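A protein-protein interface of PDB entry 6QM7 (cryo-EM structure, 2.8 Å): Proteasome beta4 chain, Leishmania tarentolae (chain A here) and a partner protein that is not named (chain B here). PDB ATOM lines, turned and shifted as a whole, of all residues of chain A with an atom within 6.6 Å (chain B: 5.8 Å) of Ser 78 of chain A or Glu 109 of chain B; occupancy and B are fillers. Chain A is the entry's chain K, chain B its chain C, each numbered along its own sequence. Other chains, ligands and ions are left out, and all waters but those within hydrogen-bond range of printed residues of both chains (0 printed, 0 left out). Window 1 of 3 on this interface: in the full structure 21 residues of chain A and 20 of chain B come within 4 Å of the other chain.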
ATOM      1  N   GLN A  43       6.216  10.754  36.571  1.00  0.00           N
ATOM      2  CA  GLN A  43       4.874  11.385  36.593  1.00  0.00           C
ATOM      3  C   GLN A  43       4.326  11.333  38.010  1.00  0.00           C
ATOM      4  O   GLN A  43       4.447  10.272  38.640  1.00  0.00           O
ATOM      5  CB  GLN A  43       3.917  10.669  35.650  1.00  0.00           C
ATOM      6  CG  GLN A  43       4.090  11.105  34.209  1.00  0.00           C
ATOM      7  CD  GLN A  43       3.317  10.264  33.234  1.00  0.00           C
ATOM      8  OE1 GLN A  43       2.381   9.544  33.587  1.00  0.00           O
ATOM      9  NE2 GLN A  43       3.738  10.345  31.987  1.00  0.00           N
ATOM     10  N   GLN A  72       0.870  -2.376  26.621  1.00  0.00           N
ATOM     11  CA  GLN A  72       1.749  -1.661  25.662  1.00  0.00           C
ATOM     12  C   GLN A  72       3.209  -2.070  25.908  1.00  0.00           C
ATOM     13  O   GLN A  72       4.098  -1.221  25.698  1.00  0.00           O
ATOM     14  CB  GLN A  72       1.508  -0.147  25.781  1.00  0.00           C
ATOM     15  CG  GLN A  72       0.103   0.279  25.346  1.00  0.00           C
ATOM     16  CD  GLN A  72      -0.355   1.640  25.819  1.00  0.00           C
ATOM     17  OE1 GLN A  72       0.445   2.537  26.068  1.00  0.00           O
ATOM     18  NE2 GLN A  72      -1.666   1.805  25.933  1.00  0.00           N
ATOM     19  N   HIS A  76       6.144   3.766  28.276  1.00  0.00           N
ATOM     20  CA  HIS A  76       5.796   4.819  29.257  1.00  0.00           C
ATOM     21  C   HIS A  76       5.083   5.943  28.511  1.00  0.00           C
ATOM     22  O   HIS A  76       5.728   6.594  27.673  1.00  0.00           O
ATOM     23  CB  HIS A  76       7.054   5.226  30.029  1.00  0.00           C
ATOM     24  CG  HIS A  76       7.416   4.214  31.069  1.00  0.00           C
ATOM     25  ND1 HIS A  76       8.046   4.551  32.251  1.00  0.00           N
ATOM     26  CD2 HIS A  76       7.182   2.883  31.134  1.00  0.00           C
ATOM     27  CE1 HIS A  76       8.210   3.467  32.985  1.00  0.00           C
ATOM     28  NE2 HIS A  76       7.684   2.432  32.325  1.00  0.00           N
ATOM     29  N   SER A  77       3.790   6.124  28.783  1.00  0.00           N
ATOM     30  CA  SER A  77       2.934   7.162  28.154  1.00  0.00           C
ATOM     31  C   SER A  77       3.435   8.554  28.540  1.00  0.00           C
ATOM     32  O   SER A  77       3.912   8.728  29.676  1.00  0.00           O
ATOM     33  CB  SER A  77       1.484   6.997  28.519  1.00  0.00           C
ATOM     34  OG  SER A  77       1.278   7.251  29.899  1.00  0.00           O
ATOM     35  N   SER A  78       3.321   9.493  27.598  1.00  0.00           N
ATOM     36  CA  SER A  78       3.654  10.933  27.738  1.00  0.00           C
ATOM     37  C   SER A  78       2.781  11.550  28.823  1.00  0.00           C
ATOM     38  O   SER A  78       1.791  10.934  29.202  1.00  0.00           O
ATOM     39  CB  SER A  78       3.449  11.647  26.434  1.00  0.00           C
ATOM     40  OG  SER A  78       2.124  11.448  25.960  1.00  0.00           O
ATOM     41  N   CYS A  79       3.119  12.756  29.257  1.00  0.00           N
ATOM     42  CA  CYS A  79       2.399  13.497  30.314  1.00  0.00           C
ATOM     43  C   CYS A  79       1.115  14.072  29.721  1.00  0.00           C
ATOM     44  O   CYS A  79       0.078  13.895  30.358  1.00  0.00           O
ATOM     45  CB  CYS A  79       3.317  14.549  30.915  1.00  0.00           C
ATOM     46  SG  CYS A  79       4.875  13.820  31.492  1.00  0.00           S
ATOM     47  N   GLU A  80       1.154  14.656  28.519  1.00  0.00           N
ATOM     48  CA  GLU A  80      -0.070  15.129  27.810  1.00  0.00           C
ATOM     49  C   GLU A  80      -1.096  13.996  27.831  1.00  0.00           C
ATOM     50  O   GLU A  80      -2.253  14.254  28.218  1.00  0.00           O
ATOM     51  CB  GLU A  80       0.202  15.552  26.362  1.00  0.00           C
ATOM     52  CG  GLU A  80       0.636  17.013  26.205  1.00  0.00           C
ATOM     53  CD  GLU A  80      -0.383  17.977  25.598  1.00  0.00           C
ATOM     54  OE1 GLU A  80      -0.090  18.553  24.515  1.00  0.00           O
ATOM     55  OE2 GLU A  80      -1.465  18.166  26.203  1.00  0.00           O
ATOM     56  N   SER A  81      -0.668  12.789  27.455  1.00  0.00           N
ATOM     57  CA  SER A  81      -1.521  11.579  27.392  1.00  0.00           C
ATOM     58  C   SER A  81      -2.181  11.321  28.748  1.00  0.00           C
ATOM     59  O   SER A  81      -3.407  11.095  28.749  1.00  0.00           O
ATOM     60  CB  SER A  81      -0.752  10.385  26.934  1.00  0.00           C
ATOM     61  OG  SER A  81      -1.524   9.195  27.026  1.00  0.00           O
ATOM     62  N   THR A  82      -1.442  11.345  29.861  1.00  0.00           N
ATOM     63  CA  THR A  82      -2.035  10.932  31.159  1.00  0.00           C
ATOM     64  C   THR A  82      -2.828  12.104  31.698  1.00  0.00           C
ATOM     65  O   THR A  82      -3.858  11.844  32.313  1.00  0.00           O
ATOM     66  CB  THR A  82      -1.074  10.322  32.189  1.00  0.00           C
ATOM     67  OG1 THR A  82      -0.801  11.167  33.305  1.00  0.00           O
ATOM     68  CG2 THR A  82       0.217   9.855  31.564  1.00  0.00           C
ATOM     69  N   ALA A  83      -2.391  13.328  31.442  1.00  0.00           N
ATOM     70  CA  ALA A  83      -3.149  14.540  31.815  1.00  0.00           C
ATOM     71  C   ALA A  83      -4.516  14.478  31.154  1.00  0.00           C
ATOM     72  O   ALA A  83      -5.504  14.744  31.838  1.00  0.00           O
ATOM     73  CB  ALA A  83      -2.409  15.789  31.406  1.00  0.00           C
ATOM     74  N   ASN A  84      -4.559  14.122  29.872  1.00  0.00           N
ATOM     75  CA  ASN A  84      -5.818  14.036  29.084  1.00  0.00           C
ATOM     76  C   ASN A  84      -6.616  12.842  29.569  1.00  0.00           C
ATOM     77  O   ASN A  84      -7.820  12.995  29.787  1.00  0.00           O
ATOM     78  CB  ASN A  84      -5.556  14.046  27.586  1.00  0.00           C
ATOM     79  CG  ASN A  84      -5.346  15.465  27.111  1.00  0.00           C
ATOM     80  OD1 ASN A  84      -6.233  16.311  27.255  1.00  0.00           O
ATOM     81  ND2 ASN A  84      -4.159  15.760  26.614  1.00  0.00           N
ATOM     82  N   PHE A 107      -0.804  17.984  37.951  1.00  0.00           N
ATOM     83  CA  PHE A 107      -0.215  16.781  37.354  1.00  0.00           C
ATOM     84  C   PHE A 107       1.111  17.208  36.750  1.00  0.00           C
ATOM     85  O   PHE A 107       1.105  17.961  35.783  1.00  0.00           O
ATOM     86  CB  PHE A 107      -1.168  16.157  36.344  1.00  0.00           C
ATOM     87  CG  PHE A 107      -0.447  15.125  35.533  1.00  0.00           C
ATOM     88  CD1 PHE A 107      -0.052  13.938  36.114  1.00  0.00           C
ATOM     89  CD2 PHE A 107      -0.078  15.389  34.233  1.00  0.00           C
ATOM     90  CE1 PHE A 107       0.680  13.010  35.388  1.00  0.00           C
ATOM     91  CE2 PHE A 107       0.659  14.466  33.516  1.00  0.00           C
ATOM     92  CZ  PHE A 107       1.046  13.279  34.093  1.00  0.00           C
ATOM     93  N   ASP A 111       8.834  14.419  30.533  1.00  0.00           N
ATOM     94  CA  ASP A 111       8.820  13.619  29.289  1.00  0.00           C
ATOM     95  C   ASP A 111      10.273  13.439  28.858  1.00  0.00           C
ATOM     96  O   ASP A 111      10.940  14.453  28.613  1.00  0.00           O
ATOM     97  CB  ASP A 111       7.943  14.280  28.223  1.00  0.00           C
ATOM     98  CG  ASP A 111       6.447  14.017  28.360  1.00  0.00           C
ATOM     99  OD1 ASP A 111       5.657  14.910  27.976  1.00  0.00           O
ATOM    100  OD2 ASP A 111       6.079  12.907  28.820  1.00  0.00           O
ATOM    101  N   VAL A 121       7.762  16.213  22.928  1.00  0.00           N
ATOM    102  CA  VAL A 121       8.229  17.113  24.028  1.00  0.00           C
ATOM    103  C   VAL A 121       9.280  16.365  24.838  1.00  0.00           C
ATOM    104  O   VAL A 121       8.991  15.242  25.284  1.00  0.00           O
ATOM    105  CB  VAL A 121       7.139  17.630  24.997  1.00  0.00           C
ATOM    106  CG1 VAL A 121       7.189  19.149  25.108  1.00  0.00           C
ATOM    107  CG2 VAL A 121       5.723  17.149  24.701  1.00  0.00           C
ATOM    108  N   ALA B 100      -8.875   4.033  16.644  1.00  0.00           N
ATOM    109  CA  ALA B 100      -7.760   4.997  16.548  1.00  0.00           C
ATOM    110  C   ALA B 100      -8.227   6.361  17.051  1.00  0.00           C
ATOM    111  O   ALA B 100      -7.459   7.015  17.772  1.00  0.00           O
ATOM    112  CB  ALA B 100      -7.233   5.084  15.139  1.00  0.00           C
ATOM    113  N   HIS B 103      -9.053   6.374  20.876  1.00  0.00           N
ATOM    114  CA  HIS B 103      -7.760   6.548  21.591  1.00  0.00           C
ATOM    115  C   HIS B 103      -7.380   8.027  21.586  1.00  0.00           C
ATOM    116  O   HIS B 103      -7.078   8.557  22.639  1.00  0.00           O
ATOM    117  CB  HIS B 103      -6.655   5.681  20.993  1.00  0.00           C
ATOM    118  CG  HIS B 103      -5.376   5.789  21.744  1.00  0.00           C
ATOM    119  ND1 HIS B 103      -4.987   4.849  22.678  1.00  0.00           N
ATOM    120  CD2 HIS B 103      -4.405   6.722  21.711  1.00  0.00           C
ATOM    121  CE1 HIS B 103      -3.819   5.200  23.184  1.00  0.00           C
ATOM    122  NE2 HIS B 103      -3.444   6.355  22.613  1.00  0.00           N
ATOM    123  N   GLN B 104      -7.404   8.664  20.425  1.00  0.00           N
ATOM    124  CA  GLN B 104      -7.068  10.097  20.294  1.00  0.00           C
ATOM    125  C   GLN B 104      -8.035  10.931  21.132  1.00  0.00           C
ATOM    126  O   GLN B 104      -7.620  11.969  21.633  1.00  0.00           O
ATOM    127  CB  GLN B 104      -7.125  10.524  18.835  1.00  0.00           C
ATOM    128  CG  GLN B 104      -6.859  12.010  18.630  1.00  0.00           C
ATOM    129  CD  GLN B 104      -6.385  12.250  17.221  1.00  0.00           C
ATOM    130  OE1 GLN B 104      -7.168  12.616  16.336  1.00  0.00           O
ATOM    131  NE2 GLN B 104      -5.105  11.975  17.005  1.00  0.00           N
ATOM    132  N   PHE B 107      -6.724  10.130  24.993  1.00  0.00           N
ATOM    133  CA  PHE B 107      -5.326  10.474  25.321  1.00  0.00           C
ATOM    134  C   PHE B 107      -4.841  11.714  24.568  1.00  0.00           C
ATOM    135  O   PHE B 107      -3.775  12.226  24.946  1.00  0.00           O
ATOM    136  CB  PHE B 107      -4.448   9.257  25.056  1.00  0.00           C
ATOM    137  CG  PHE B 107      -4.865   8.074  25.888  1.00  0.00           C
ATOM    138  CD1 PHE B 107      -4.468   7.965  27.211  1.00  0.00           C
ATOM    139  CD2 PHE B 107      -5.716   7.113  25.381  1.00  0.00           C
ATOM    140  CE1 PHE B 107      -4.889   6.912  28.004  1.00  0.00           C
ATOM    141  CE2 PHE B 107      -6.145   6.061  26.172  1.00  0.00           C
ATOM    142  CZ  PHE B 107      -5.732   5.964  27.482  1.00  0.00           C
ATOM    143  N   GLN B 108      -5.572  12.212  23.572  1.00  0.00           N
ATOM    144  CA  GLN B 108      -5.169  13.398  22.758  1.00  0.00           C
ATOM    145  C   GLN B 108      -3.750  13.186  22.236  1.00  0.00           C
ATOM    146  O   GLN B 108      -2.975  14.150  22.210  1.00  0.00           O
ATOM    147  CB  GLN B 108      -5.323  14.700  23.550  1.00  0.00           C
ATOM    148  CG  GLN B 108      -6.776  15.036  23.882  1.00  0.00           C
ATOM    149  CD  GLN B 108      -7.660  15.126  22.656  1.00  0.00           C
ATOM    150  OE1 GLN B 108      -7.307  15.760  21.658  1.00  0.00           O
ATOM    151  NE2 GLN B 108      -8.816  14.482  22.711  1.00  0.00           N
ATOM    152  N   GLU B 109      -3.448  11.955  21.830  1.00  0.00           N
ATOM    153  CA  GLU B 109      -2.195  11.589  21.137  1.00  0.00           C
ATOM    154  C   GLU B 109      -2.522  10.486  20.144  1.00  0.00           C
ATOM    155  O   GLU B 109      -3.509   9.788  20.308  1.00  0.00           O
ATOM    156  CB  GLU B 109      -1.120  11.152  22.134  1.00  0.00           C
ATOM    157  CG  GLU B 109      -1.511   9.949  22.979  1.00  0.00           C
ATOM    158  CD  GLU B 109      -0.388   8.983  23.345  1.00  0.00           C
ATOM    159  OE1 GLU B 109      -0.700   7.785  23.590  1.00  0.00           O
ATOM    160  OE2 GLU B 109       0.792   9.421  23.404  1.00  0.00           O
ATOM    161  N   PRO B 110      -1.735  10.312  19.066  1.00  0.00           N
ATOM    162  CA  PRO B 110      -1.957   9.210  18.137  1.00  0.00           C
ATOM    163  C   PRO B 110      -1.732   7.850  18.804  1.00  0.00           C
ATOM    164  O   PRO B 110      -0.779   7.694  19.538  1.00  0.00           O
ATOM    165  CB  PRO B 110      -0.931   9.439  17.026  1.00  0.00           C
ATOM    166  CG  PRO B 110       0.133  10.273  17.698  1.00  0.00           C
ATOM    167  CD  PRO B 110      -0.624  11.174  18.649  1.00  0.00           C
ATOM    168  N   MET B 111      -2.656   6.929  18.544  1.00  0.00           N
ATOM    169  CA  MET B 111      -2.589   5.516  18.975  1.00  0.00           C
ATOM    170  C   MET B 111      -1.322   4.886  18.416  1.00  0.00           C
ATOM    171  O   MET B 111      -1.043   5.069  17.214  1.00  0.00           O
ATOM    172  CB  MET B 111      -3.786   4.735  18.433  1.00  0.00           C
ATOM    173  CG  MET B 111      -4.020   3.462  19.174  1.00  0.00           C
ATOM    174  SD  MET B 111      -5.568   2.742  18.687  1.00  0.00           S
ATOM    175  CE  MET B 111      -5.995   1.856  20.188  1.00  0.00           C
ATOM    176  N   ALA B 112      -0.596   4.146  19.241  1.00  0.00           N
ATOM    177  CA  ALA B 112       0.534   3.320  18.776  1.00  0.00           C
ATOM    178  C   ALA B 112       0.014   2.285  17.778  1.00  0.00           C
ATOM    179  O   ALA B 112      -1.117   1.824  17.933  1.00  0.00           O
ATOM    180  CB  ALA B 112       1.188   2.648  19.941  1.00  0.00           C
ATOM    181  N   ARG B 147       5.893   7.293  17.896  1.00  0.00           N
ATOM    182  CA  ARG B 147       7.147   7.760  18.538  1.00  0.00           C
ATOM    183  C   ARG B 147       7.830   6.582  19.238  1.00  0.00           C
ATOM    184  O   ARG B 147       9.030   6.690  19.498  1.00  0.00           O
ATOM    185  CB  ARG B 147       6.922   8.974  19.452  1.00  0.00           C
ATOM    186  CG  ARG B 147       5.743   8.926  20.417  1.00  0.00           C
ATOM    187  CD  ARG B 147       5.630  10.221  21.220  1.00  0.00           C
ATOM    188  NE  ARG B 147       6.165  10.098  22.572  1.00  0.00           N
ATOM    189  CZ  ARG B 147       5.555   9.499  23.603  1.00  0.00           C
ATOM    190  NH1 ARG B 147       6.158   9.447  24.780  1.00  0.00           N
ATOM    191  NH2 ARG B 147       4.360   8.944  23.462  1.00  0.00           N
ATOM    192  N   TYR B 148       7.122   5.484  19.480  1.00  0.00           N
ATOM    193  CA  TYR B 148       7.640   4.342  20.266  1.00  0.00           C
ATOM    194  C   TYR B 148       8.620   3.547  19.411  1.00  0.00           C
ATOM    195  O   TYR B 148       9.791   3.478  19.796  1.00  0.00           O
ATOM    196  CB  TYR B 148       6.486   3.504  20.815  1.00  0.00           C
ATOM    197  CG  TYR B 148       5.561   4.276  21.726  1.00  0.00           C
ATOM    198  CD1 TYR B 148       5.989   4.713  22.971  1.00  0.00           C
ATOM    199  CD2 TYR B 148       4.263   4.591  21.344  1.00  0.00           C
ATOM    200  CE1 TYR B 148       5.151   5.419  23.821  1.00  0.00           C
ATOM    201  CE2 TYR B 148       3.412   5.298  22.182  1.00  0.00           C
ATOM    202  CZ  TYR B 148       3.856   5.712  23.428  1.00  0.00           C
ATOM    203  OH  TYR B 148       3.030   6.410  24.265  1.00  0.00           O
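Hydrophobic or aromatic side chains of chain B within 4 Å of the printed part of chain A: Phe 107 and Tyr 148. Among the printed residues, 7 pairs touch across the chains. Among the printed residues, no Asp or Glu carboxylate lies within 4 Å of a Lys or Arg side-chain nitrogen of the other chain.
Gln 43 of chain A touches none of the printed residues of chain B. Printed residues of chain B within 4 Å of Ser 77 of chain A: Tyr 148. Of the printed residues of chain B, Asn 84 of chain A touches Phe 107 and Gln 108. His 103 of chain B touches none of the printed residues of chain A. Printed residues of chain A within 4 Å of Phe 107 of chain B: Ser 81 and Asn 84. Glu 109 of chain B touches just these residues of chain A: Ser 78 and Ser 81. Of the printed residues of chain A, Tyr 148 of chain B touches Ser 77.
OH of Tyr 148 of chain B touches CA of Ser 77 of chain A (3.96 Å). Glu 109 of chain B touches Ser 78 of chain A. CB of Ser 78 of chain A touches NH1 of Arg 147 of chain B, 3.9 Å away. CD1 of Phe 107 of chain B touches OG of Ser 81 of chain A, at 3.2 Å. Ser 81 of chain A touches Glu 109 of chain B. Asn 84 of chain A touches Phe 107 of chain B. ND2 of Asn 84 of chain A touches CB of Gln 108 of chain B, 3.4 Å away.
NE2 of Gln 43 of chain A sits at hydrogen-bond distance from O of Ser 78 of chain A, at 3.4 Å. The side-chain hydroxyl (OG) of Ser 78 of chain A sits close to the backbone NH (N) of Ser 81 of chain A, at 3.4 Å. The side-chain amide nitrogen (ND2) of Asn 84 of chain A sits at hydrogen-bond distance from the backbone carbonyl oxygen (O) of Glu 80 of chain A (2.9 Å). O of Gln 104 of chain B sits at hydrogen-bond distance from NE2 of Gln 108 of chain B. The side-chain carboxylate (OE2) of Glu 109 of chain B is in salt-bridge range of the guanidinium group (NH2) of Arg 147 of chain B (3.6 Å). The side-chain hydroxyl (OH) of Tyr 148 of chain B lies within hydrogen-bond range of the guanidinium group (NH2) of Arg 147 of chain B.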
